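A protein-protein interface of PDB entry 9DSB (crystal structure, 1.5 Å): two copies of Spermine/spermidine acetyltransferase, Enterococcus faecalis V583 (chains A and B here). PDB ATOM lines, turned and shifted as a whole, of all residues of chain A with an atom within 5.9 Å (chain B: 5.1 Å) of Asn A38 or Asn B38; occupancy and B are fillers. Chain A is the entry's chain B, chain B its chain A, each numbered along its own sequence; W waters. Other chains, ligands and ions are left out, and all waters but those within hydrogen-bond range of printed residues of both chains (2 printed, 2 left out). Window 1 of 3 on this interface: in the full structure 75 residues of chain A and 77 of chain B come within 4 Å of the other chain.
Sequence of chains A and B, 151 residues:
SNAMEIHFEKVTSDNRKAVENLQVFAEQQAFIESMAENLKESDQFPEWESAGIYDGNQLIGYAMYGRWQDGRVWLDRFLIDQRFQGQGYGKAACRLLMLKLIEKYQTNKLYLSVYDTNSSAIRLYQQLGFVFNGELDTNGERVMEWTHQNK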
ATOM      1  N   GLU A  33     -16.346  -2.692  13.223  1.00  0.00           N
ATOM      2  CA  GLU A  33     -14.994  -2.479  13.713  1.00  0.00           C
ATOM      3  C   GLU A  33     -13.967  -3.057  12.742  1.00  0.00           C
ATOM      4  O   GLU A  33     -12.926  -2.446  12.520  1.00  0.00           O
ATOM      5  CB  GLU A  33     -14.811  -3.063  15.113  1.00  0.00           C
ATOM      6  CG  GLU A  33     -15.742  -2.433  16.141  1.00  0.00           C
ATOM      7  CD  GLU A  33     -15.599  -0.929  16.305  1.00  0.00           C
ATOM      8  OE1 GLU A  33     -14.621  -0.343  15.792  1.00  0.00           O
ATOM      9  OE2 GLU A  33     -16.488  -0.330  16.945  1.00  0.00           O
ATOM     10  N   SER A  34     -14.244  -4.248  12.203  1.00  0.00           N
ATOM     11  CA  SER A  34     -13.339  -4.871  11.252  1.00  0.00           C
ATOM     12  C   SER A  34     -13.145  -3.958  10.043  1.00  0.00           C
ATOM     13  O   SER A  34     -12.017  -3.737   9.610  1.00  0.00           O
ATOM     14  CB  SER A  34     -13.832  -6.222  10.828  1.00  0.00           C
ATOM     15  OG  SER A  34     -13.891  -7.109  11.935  1.00  0.00           O
ATOM     16  N   MET A  35     -14.252  -3.429   9.510  1.00  0.00           N
ATOM     17  CA  MET A  35     -14.202  -2.559   8.343  1.00  0.00           C
ATOM     18  C   MET A  35     -13.507  -1.243   8.683  1.00  0.00           C
ATOM     19  O   MET A  35     -12.714  -0.742   7.895  1.00  0.00           O
ATOM     20  CB  MET A  35     -15.601  -2.275   7.784  1.00  0.00           C
ATOM     21  CG  MET A  35     -15.597  -1.408   6.528  1.00  0.00           C
ATOM     22  SD  MET A  35     -14.793  -2.117   5.077  1.00  0.00           S
ATOM     23  CE  MET A  35     -15.896  -3.501   4.760  1.00  0.00           C
ATOM     24  N   ALA A  36     -13.800  -0.681   9.861  1.00  0.00           N
ATOM     25  CA  ALA A  36     -13.161   0.553  10.289  1.00  0.00           C
ATOM     26  C   ALA A  36     -11.645   0.384  10.339  1.00  0.00           C
ATOM     27  O   ALA A  36     -10.903   1.279   9.939  1.00  0.00           O
ATOM     28  CB  ALA A  36     -13.713   0.987  11.622  1.00  0.00           C
ATOM     29  N   GLU A  37     -11.198  -0.781  10.819  1.00  0.00           N
ATOM     30  CA  GLU A  37      -9.780  -1.086  10.913  1.00  0.00           C
ATOM     31  C   GLU A  37      -9.194  -1.280   9.514  1.00  0.00           C
ATOM     32  O   GLU A  37      -8.050  -0.917   9.277  1.00  0.00           O
ATOM     33  CB  GLU A  37      -9.527  -2.307  11.798  1.00  0.00           C
ATOM     34  CG  GLU A  37      -8.050  -2.675  11.909  1.00  0.00           C
ATOM     35  CD  GLU A  37      -7.170  -1.621  12.551  1.00  0.00           C
ATOM     36  OE1 GLU A  37      -7.703  -0.731  13.248  1.00  0.00           O
ATOM     37  OE2 GLU A  37      -5.939  -1.697  12.352  1.00  0.00           O
ATOM     38  N   ASN A  38      -9.978  -1.850   8.590  1.00  0.00           N
ATOM     39  CA  ASN A  38      -9.545  -1.990   7.206  1.00  0.00           C
ATOM     40  C   ASN A  38      -9.217  -0.613   6.631  1.00  0.00           C
ATOM     41  O   ASN A  38      -8.185  -0.428   5.989  1.00  0.00           O
ATOM     42  CB  ASN A  38     -10.603  -2.644   6.321  1.00  0.00           C
ATOM     43  CG  ASN A  38     -10.879  -4.085   6.672  1.00  0.00           C
ATOM     44  OD1 ASN A  38     -10.075  -4.732   7.356  1.00  0.00           O
ATOM     45  ND2 ASN A  38     -12.006  -4.603   6.201  1.00  0.00           N
ATOM     46  N   LEU A  39     -10.118   0.344   6.871  1.00  0.00           N
ATOM     47  CA  LEU A  39      -9.984   1.697   6.349  1.00  0.00           C
ATOM     48  C   LEU A  39      -8.798   2.407   6.994  1.00  0.00           C
ATOM     49  O   LEU A  39      -8.114   3.185   6.335  1.00  0.00           O
ATOM     50  CB  LEU A  39     -11.276   2.483   6.558  1.00  0.00           C
ATOM     51  CG  LEU A  39     -12.524   1.937   5.863  1.00  0.00           C
ATOM     52  CD1 LEU A  39     -13.726   2.813   6.186  1.00  0.00           C
ATOM     53  CD2 LEU A  39     -12.323   1.837   4.366  1.00  0.00           C
ATOM     54  N   LYS A  40      -8.574   2.165   8.289  1.00  0.00           N
ATOM     55  CA  LYS A  40      -7.457   2.779   8.987  1.00  0.00           C
ATOM     56  C   LYS A  40      -6.140   2.323   8.364  1.00  0.00           C
ATOM     57  O   LYS A  40      -5.275   3.146   8.067  1.00  0.00           O
ATOM     58  CB  LYS A  40      -7.492   2.439  10.479  1.00  0.00           C
ATOM     59  CG  LYS A  40      -6.329   3.009  11.278  1.00  0.00           C
ATOM     60  CD  LYS A  40      -6.468   2.833  12.784  1.00  0.00           C
ATOM     61  CE  LYS A  40      -5.276   3.353  13.520  1.00  0.00           C
ATOM     62  NZ  LYS A  40      -5.422   3.188  14.965  1.00  0.00           N
ATOM     63  N   GLU A  41      -6.012   1.006   8.165  1.00  0.00           N
ATOM     64  CA  GLU A  41      -4.781   0.410   7.673  1.00  0.00           C
ATOM     65  C   GLU A  41      -4.550   0.830   6.223  1.00  0.00           C
ATOM     66  O   GLU A  41      -3.424   1.131   5.838  1.00  0.00           O
ATOM     67  CB  GLU A  41      -4.820  -1.110   7.836  1.00  0.00           C
ATOM     68  CG  GLU A  41      -4.888  -1.551   9.296  1.00  0.00           C
ATOM     69  CD  GLU A  41      -4.842  -3.053   9.521  1.00  0.00           C
ATOM     70  OE1 GLU A  41      -4.576  -3.800   8.554  1.00  0.00           O
ATOM     71  OE2 GLU A  41      -5.098  -3.483  10.665  1.00  0.00           O
ATOM     72  N   SER A  42      -5.632   0.865   5.440  1.00  0.00           N
ATOM     73  CA  SER A  42      -5.559   1.290   4.051  1.00  0.00           C
ATOM     74  C   SER A  42      -5.074   2.733   3.954  1.00  0.00           C
ATOM     75  O   SER A  42      -4.196   3.036   3.146  1.00  0.00           O
ATOM     76  CB  SER A  42      -6.882   1.117   3.359  1.00  0.00           C
ATOM     77  OG  SER A  42      -6.736   1.342   1.965  1.00  0.00           O
ATOM     78  N   ASP A  43      -5.653   3.614   4.781  1.00  0.00           N
ATOM     79  CA  ASP A  43      -5.354   5.038   4.748  1.00  0.00           C
ATOM     80  C   ASP A  43      -3.927   5.300   5.224  1.00  0.00           C
ATOM     81  O   ASP A  43      -3.346   6.334   4.897  1.00  0.00           O
ATOM     82  CB  ASP A  43      -6.368   5.832   5.557  1.00  0.00           C
ATOM     83  CG  ASP A  43      -7.793   5.790   5.027  1.00  0.00           C
ATOM     84  OD1 ASP A  43      -8.012   5.143   3.984  1.00  0.00           O
ATOM     85  OD2 ASP A  43      -8.677   6.392   5.665  1.00  0.00           O
ATOM     86  N   SER A  50      -8.518   2.271  -0.663  1.00  0.00           N
ATOM     87  CA  SER A  50      -9.865   1.781  -0.424  1.00  0.00           C
ATOM     88  C   SER A  50     -10.851   2.594  -1.259  1.00  0.00           C
ATOM     89  O   SER A  50     -10.686   3.805  -1.418  1.00  0.00           O
ATOM     90  CB  SER A  50     -10.220   1.863   1.046  1.00  0.00           C
ATOM     91  OG  SER A  50      -9.623   0.816   1.802  1.00  0.00           O
ATOM     92  N   TYR A  62     -17.370  -2.684  -1.393  1.00  0.00           N
ATOM     93  CA  TYR A  62     -16.097  -2.134  -0.966  1.00  0.00           C
ATOM     94  C   TYR A  62     -14.965  -2.869  -1.674  1.00  0.00           C
ATOM     95  O   TYR A  62     -15.008  -4.093  -1.843  1.00  0.00           O
ATOM     96  CB  TYR A  62     -15.968  -2.271   0.552  1.00  0.00           C
ATOM     97  CG  TYR A  62     -14.558  -2.111   1.099  1.00  0.00           C
ATOM     98  CD1 TYR A  62     -13.978  -0.856   1.251  1.00  0.00           C
ATOM     99  CD2 TYR A  62     -13.824  -3.215   1.514  1.00  0.00           C
ATOM    100  CE1 TYR A  62     -12.699  -0.711   1.768  1.00  0.00           C
ATOM    101  CE2 TYR A  62     -12.546  -3.081   2.026  1.00  0.00           C
ATOM    102  CZ  TYR A  62     -11.983  -1.826   2.164  1.00  0.00           C
ATOM    103  OH  TYR A  62     -10.724  -1.713   2.691  1.00  0.00           O
ATOM    104  N   MET A  64     -10.435  -2.889  -1.883  1.00  0.00           N
ATOM    105  CA  MET A  64      -9.122  -2.429  -1.470  1.00  0.00           C
ATOM    106  C   MET A  64      -8.095  -3.067  -2.402  1.00  0.00           C
ATOM    107  O   MET A  64      -8.171  -4.264  -2.677  1.00  0.00           O
ATOM    108  CB  MET A  64      -8.835  -2.806  -0.014  1.00  0.00           C
ATOM    109  CG  MET A  64      -7.518  -2.282   0.504  1.00  0.00           C
ATOM    110  SD  MET A  64      -7.281  -2.618   2.261  1.00  0.00           S
ATOM    111  CE  MET A  64      -5.491  -2.471   2.344  1.00  0.00           C
ATOM    112  N   ARG A  77      -9.093  -6.712  -1.153  1.00  0.00           N
ATOM    113  CA  ARG A  77     -10.369  -6.905  -0.489  1.00  0.00           C
ATOM    114  C   ARG A  77     -11.462  -6.561  -1.494  1.00  0.00           C
ATOM    115  O   ARG A  77     -11.303  -5.630  -2.276  1.00  0.00           O
ATOM    116  CB  ARG A  77     -10.462  -6.010   0.755  1.00  0.00           C
ATOM    117  CG  ARG A  77      -9.378  -6.204   1.811  1.00  0.00           C
ATOM    118  CD  ARG A  77      -9.586  -5.283   3.006  1.00  0.00           C
ATOM    119  NE  ARG A  77      -8.620  -5.448   4.098  1.00  0.00           N
ATOM    120  CZ  ARG A  77      -8.594  -6.408   5.024  1.00  0.00           C
ATOM    121  NH1 ARG A  77      -9.512  -7.360   5.071  1.00  0.00           N
ATOM    122  NH2 ARG A  77      -7.635  -6.414   5.933  1.00  0.00           N
ATOM    123  N   LEU A  79     -15.889  -6.885  -1.540  1.00  0.00           N
ATOM    124  CA  LEU A  79     -17.107  -7.262  -0.842  1.00  0.00           C
ATOM    125  C   LEU A  79     -18.297  -6.609  -1.531  1.00  0.00           C
ATOM    126  O   LEU A  79     -18.245  -5.427  -1.866  1.00  0.00           O
ATOM    127  CB  LEU A  79     -17.080  -6.822   0.621  1.00  0.00           C
ATOM    128  CG  LEU A  79     -16.038  -7.480   1.526  1.00  0.00           C
ATOM    129  CD1 LEU A  79     -16.035  -6.729   2.845  1.00  0.00           C
ATOM    130  CD2 LEU A  79     -16.309  -8.960   1.752  1.00  0.00           C
ATOM    131  N   GLU B  33     -11.982 -14.724   3.493  1.00  0.00           N
ATOM    132  CA  GLU B  33     -11.075 -13.918   2.691  1.00  0.00           C
ATOM    133  C   GLU B  33     -10.661 -12.673   3.472  1.00  0.00           C
ATOM    134  O   GLU B  33      -9.512 -12.247   3.384  1.00  0.00           O
ATOM    135  CB  GLU B  33     -11.701 -13.550   1.345  1.00  0.00           C
ATOM    136  CG  GLU B  33     -12.065 -14.761   0.490  1.00  0.00           C
ATOM    137  CD  GLU B  33     -10.890 -15.633   0.087  1.00  0.00           C
ATOM    138  OE1 GLU B  33      -9.731 -15.186   0.230  1.00  0.00           O
ATOM    139  OE2 GLU B  33     -11.134 -16.785  -0.339  1.00  0.00           O
ATOM    140  N   SER B  34     -11.596 -12.086   4.227  1.00  0.00           N
ATOM    141  CA  SER B  34     -11.287 -10.913   5.028  1.00  0.00           C
ATOM    142  C   SER B  34     -10.185 -11.227   6.034  1.00  0.00           C
ATOM    143  O   SER B  34      -9.258 -10.440   6.210  1.00  0.00           O
ATOM    144  CB  SER B  34     -12.506 -10.370   5.734  1.00  0.00           C
ATOM    145  OG  SER B  34     -12.490  -8.944   5.743  1.00  0.00           O
ATOM    146  N   MET B  35     -10.299 -12.384   6.690  1.00  0.00           N
ATOM    147  CA  MET B  35      -9.342 -12.767   7.715  1.00  0.00           C
ATOM    148  C   MET B  35      -7.992 -13.078   7.073  1.00  0.00           C
ATOM    149  O   MET B  35      -6.953 -12.694   7.602  1.00  0.00           O
ATOM    150  CB  MET B  35      -9.845 -13.963   8.528  1.00  0.00           C
ATOM    151  CG  MET B  35      -8.967 -14.308   9.724  1.00  0.00           C
ATOM    152  SD  MET B  35      -8.692 -12.969  10.902  1.00  0.00           S
ATOM    153  CE  MET B  35     -10.384 -12.580  11.367  1.00  0.00           C
ATOM    154  N   ALA B  36      -8.008 -13.782   5.932  1.00  0.00           N
ATOM    155  CA  ALA B  36      -6.777 -14.114   5.234  1.00  0.00           C
ATOM    156  C   ALA B  36      -6.010 -12.842   4.881  1.00  0.00           C
ATOM    157  O   ALA B  36      -4.790 -12.790   4.994  1.00  0.00           O
ATOM    158  CB  ALA B  36      -7.077 -14.951   4.013  1.00  0.00           C
ATOM    159  N   GLU B  37      -6.733 -11.802   4.465  1.00  0.00           N
ATOM    160  CA  GLU B  37      -6.100 -10.533   4.149  1.00  0.00           C
ATOM    161  C   GLU B  37      -5.639  -9.860   5.442  1.00  0.00           C
ATOM    162  O   GLU B  37      -4.538  -9.321   5.482  1.00  0.00           O
ATOM    163  CB  GLU B  37      -7.018  -9.654   3.301  1.00  0.00           C
ATOM    164  CG  GLU B  37      -6.383  -8.325   2.901  1.00  0.00           C
ATOM    165  CD  GLU B  37      -5.126  -8.400   2.052  1.00  0.00           C
ATOM    166  OE1 GLU B  37      -4.874  -9.470   1.471  1.00  0.00           O
ATOM    167  OE2 GLU B  37      -4.391  -7.388   1.971  1.00  0.00           O
ATOM    168  N   ASN B  38      -6.478  -9.886   6.492  1.00  0.00           N
ATOM    169  CA  ASN B  38      -6.085  -9.364   7.795  1.00  0.00           C
ATOM    170  C   ASN B  38      -4.721  -9.931   8.184  1.00  0.00           C
ATOM    171  O   ASN B  38      -3.828  -9.188   8.590  1.00  0.00           O
ATOM    172  CB  ASN B  38      -7.071  -9.695   8.915  1.00  0.00           C
ATOM    173  CG  ASN B  38      -8.378  -8.946   8.818  1.00  0.00           C
ATOM    174  OD1 ASN B  38      -8.495  -7.978   8.058  1.00  0.00           O
ATOM    175  ND2 ASN B  38      -9.361  -9.370   9.600  1.00  0.00           N
ATOM    176  N   LEU B  39      -4.581 -11.253   8.061  1.00  0.00           N
ATOM    177  CA  LEU B  39      -3.369 -11.939   8.481  1.00  0.00           C
ATOM    178  C   LEU B  39      -2.212 -11.529   7.575  1.00  0.00           C
ATOM    179  O   LEU B  39      -1.120 -11.232   8.047  1.00  0.00           O
ATOM    180  CB  LEU B  39      -3.587 -13.450   8.483  1.00  0.00           C
ATOM    181  CG  LEU B  39      -4.535 -14.001   9.554  1.00  0.00           C
ATOM    182  CD1 LEU B  39      -4.744 -15.493   9.332  1.00  0.00           C
ATOM    183  CD2 LEU B  39      -4.019 -13.743  10.958  1.00  0.00           C
ATOM    184  N   LYS B  40      -2.467 -11.467   6.269  1.00  0.00           N
ATOM    185  CA  LYS B  40      -1.442 -11.071   5.321  1.00  0.00           C
ATOM    186  C   LYS B  40      -0.906  -9.676   5.641  1.00  0.00           C
ATOM    187  O   LYS B  40       0.301  -9.452   5.584  1.00  0.00           O
ATOM    188  CB  LYS B  40      -2.035 -11.118   3.914  1.00  0.00           C
ATOM    189  CG  LYS B  40      -1.036 -10.838   2.809  1.00  0.00           C
ATOM    190  CD  LYS B  40      -1.661 -10.933   1.426  1.00  0.00           C
ATOM    191  CE  LYS B  40      -0.646 -10.760   0.356  1.00  0.00           C
ATOM    192  NZ  LYS B  40      -1.290 -10.812  -0.958  1.00  0.00           N
ATOM    193  N   GLU B  41      -1.811  -8.747   5.970  1.00  0.00           N
ATOM    194  CA  GLU B  41      -1.437  -7.361   6.213  1.00  0.00           C
ATOM    195  C   GLU B  41      -0.607  -7.257   7.491  1.00  0.00           C
ATOM    196  O   GLU B  41       0.331  -6.465   7.541  1.00  0.00           O
ATOM    197  CB  GLU B  41      -2.676  -6.465   6.225  1.00  0.00           C
ATOM    198  CG  GLU B  41      -3.290  -6.319   4.837  1.00  0.00           C
ATOM    199  CD  GLU B  41      -4.544  -5.471   4.742  1.00  0.00           C
ATOM    200  OE1 GLU B  41      -4.907  -4.807   5.736  1.00  0.00           O
ATOM    201  OE2 GLU B  41      -5.170  -5.509   3.663  1.00  0.00           O
ATOM    202  N   SER B  42      -0.947  -8.056   8.512  1.00  0.00           N
ATOM    203  CA  SER B  42      -0.172  -8.078   9.745  1.00  0.00           C
ATOM    204  C   SER B  42       1.219  -8.658   9.494  1.00  0.00           C
ATOM    205  O   SER B  42       2.206  -8.128   9.999  1.00  0.00           O
ATOM    206  CB  SER B  42      -0.885  -8.816  10.858  1.00  0.00           C
ATOM    207  OG  SER B  42      -0.844 -10.227  10.694  1.00  0.00           O
ATOM    208  N   SER B  50      -0.447 -10.538  14.691  1.00  0.00           N
ATOM    209  CA  SER B  50      -1.699 -11.249  14.874  1.00  0.00           C
ATOM    210  C   SER B  50      -1.491 -12.374  15.883  1.00  0.00           C
ATOM    211  O   SER B  50      -0.391 -12.915  15.993  1.00  0.00           O
ATOM    212  CB  SER B  50      -2.206 -11.788  13.553  1.00  0.00           C
ATOM    213  OG  SER B  50      -2.695 -10.755  12.706  1.00  0.00           O
ATOM    214  N   TYR B  62      -9.422 -14.155  18.024  1.00  0.00           N
ATOM    215  CA  TYR B  62      -8.341 -13.556  17.268  1.00  0.00           C
ATOM    216  C   TYR B  62      -8.121 -12.129  17.751  1.00  0.00           C
ATOM    217  O   TYR B  62      -9.069 -11.448  18.150  1.00  0.00           O
ATOM    218  CB  TYR B  62      -8.721 -13.558  15.788  1.00  0.00           C
ATOM    219  CG  TYR B  62      -7.842 -12.688  14.901  1.00  0.00           C
ATOM    220  CD1 TYR B  62      -6.566 -13.104  14.542  1.00  0.00           C
ATOM    221  CD2 TYR B  62      -8.298 -11.474  14.395  1.00  0.00           C
ATOM    222  CE1 TYR B  62      -5.763 -12.333  13.719  1.00  0.00           C
ATOM    223  CE2 TYR B  62      -7.499 -10.690  13.577  1.00  0.00           C
ATOM    224  CZ  TYR B  62      -6.231 -11.127  13.231  1.00  0.00           C
ATOM    225  OH  TYR B  62      -5.439 -10.367  12.419  1.00  0.00           O
ATOM    226  N   MET B  64      -5.374  -8.586  16.712  1.00  0.00           N
ATOM    227  CA  MET B  64      -4.212  -7.945  16.125  1.00  0.00           C
ATOM    228  C   MET B  64      -3.885  -6.709  16.955  1.00  0.00           C
ATOM    229  O   MET B  64      -4.786  -6.041  17.466  1.00  0.00           O
ATOM    230  CB  MET B  64      -4.439  -7.529  14.667  1.00  0.00           C
ATOM    231  CG  MET B  64      -3.171  -7.050  13.980  1.00  0.00           C
ATOM    232  SD  MET B  64      -3.451  -6.317  12.357  1.00  0.00           S
ATOM    233  CE  MET B  64      -4.284  -7.669  11.517  1.00  0.00           C
ATOM    234  N   ARG B  77      -7.438  -5.161  16.241  1.00  0.00           N
ATOM    235  CA  ARG B  77      -8.563  -6.051  16.011  1.00  0.00           C
ATOM    236  C   ARG B  77      -8.707  -6.983  17.209  1.00  0.00           C
ATOM    237  O   ARG B  77      -7.708  -7.356  17.807  1.00  0.00           O
ATOM    238  CB  ARG B  77      -8.346  -6.909  14.756  1.00  0.00           C
ATOM    239  CG  ARG B  77      -8.103  -6.122  13.475  1.00  0.00           C
ATOM    240  CD  ARG B  77      -7.787  -7.043  12.309  1.00  0.00           C
ATOM    241  NE  ARG B  77      -7.458  -6.310  11.083  1.00  0.00           N
ATOM    242  CZ  ARG B  77      -8.327  -5.684  10.291  1.00  0.00           C
ATOM    243  NH1 ARG B  77      -9.629  -5.749  10.521  1.00  0.00           N
ATOM    244  NH2 ARG B  77      -7.900  -5.018   9.231  1.00  0.00           N
HETATM  245  O   HOH W   1     -10.960  -7.362  12.586  1.00  0.00           O
HETATM  246  O   HOH W   2     -11.298  -7.483   7.983  1.00  0.00           O
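The guanidinium group (NH1) of Arg A77 lies within hydrogen-bond range of the backbone carbonyl oxygen (O) of Ser B34, at 3.3 Å. The guanidinium group (NH2) of Arg A77 lies within hydrogen-bond range of the side-chain amide oxygen (OD1) of Asn B38, at 2.8 Å. OE1 of Glu B41 lies within salt-bridge range of NH2 of Arg A77, 3.2 Å away. O of Ser A34 sits at hydrogen-bond distance from NH1 of Arg B77 (3.3 Å). NH2 of Arg B77 lies within hydrogen-bond range of OD1 of Asn A38. The guanidinium group (NH2) of Arg B77 lies within salt-bridge range of the side-chain carboxylate (OE2) of Glu A41 (3.5 Å). OE1 of Glu A41 sits close to OE1 of Glu B41, 3.0 Å away. The side-chain sulfur of Met B64 lies close to the side-chain carboxylate of Glu A41, 3.7 Å away.
The side-chain amide oxygen of Asn B38 lies close to the backbone carbonyl oxygen of Ser B34 (3.2 Å). OE2 of Glu B41 sits close to OE2 of Glu B37 (2.6 Å). The backbone NH of Met B64 lies within hydrogen-bond range of the backbone carbonyl oxygen of Arg B77 (2.9 Å). O of Ser A34 sits close to OD1 of Asn A38, 3.1 Å away. OE2 of Glu A37 lies close to OE2 of Glu A41 (2.6 Å). The side-chain amide oxygen of Asn A38 sits close to the guanidinium group of Arg A77, at 3.3 Å.
Among the printed residues, pairs that only touch across the chains: Met A64 with Glu B41 (3.3 Å), Glu A37 with Arg B77 (3.4 Å), Arg A77 with Arg B77 (3.6 Å), Arg A77 with Glu B37 (3.6 Å) and Asn A38 with Asn B38 (3.7 Å).
Of chain B, only Asn B38 and Arg B77 come within 4 Å of Asn A38. Printed residues of chain B within 4 Å of Glu A41: Glu B41, Met B64 and Arg B77. Of the printed residues of chain A, Met B64 touches Glu A41. Printed residues of chain B within 4 Å of Glu A37: Arg B77. The nearest residue of chain B that does not touch Asn A38 is Ser B34 (4.4 Å).
Of the 14 printed residues of chain B, 6 touch a printed residue of chain A. Printed residues of chain B that touch a printed residue of chain A: Ser B34, Glu B37, Asn B38, Glu B41, Met B64 and Arg B77. Hydrophobic or aromatic side chains of chain B that line the printed part of chain A: Met B64. Of the 16 printed residues of chain A, 6 touch a printed residue of chain B. Among the printed residues, 13 pairs touch across the chains. Among the printed residues, Asp or Glu carboxylates within 4 Å of a Lys or Arg side-chain nitrogen of the other chain: Glu A41 with Arg B77 (3.5 Å) and Arg A77 with Glu B41 (3.2 Å).
Glu A37 touches Arg B77, and with the chains exchanged Arg A77 touches Glu B37. Asn A38 touches Arg B77, and with the chains exchanged Arg A77 touches Asn B38. Glu A41 touches Met B64, and with the chains exchanged Met A64 touches Glu B41. Glu A41 touches Arg B77, and with the chains exchanged Arg A77 touches Glu B41. Positions printed for both chains: 33, 34, 35, 36, 37, 38, 39, 40, 41, 42, 50, 62, 64 and 77. Of the 13 pairs that touch across the chains among the printed residues, 13 have their exchanged pair printed and touching as well.
Water W2 lies within hydrogen-bond range of OD1 of Asn B38, OG of Ser B34, OD1 of Asn A38, NH1 of Arg A77 and NH1 of Arg B77. Water W1 lies within hydrogen-bond range of the guanidinium group (NH1) of Arg B77 and the side-chain hydroxyl (OG) of Ser A34.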
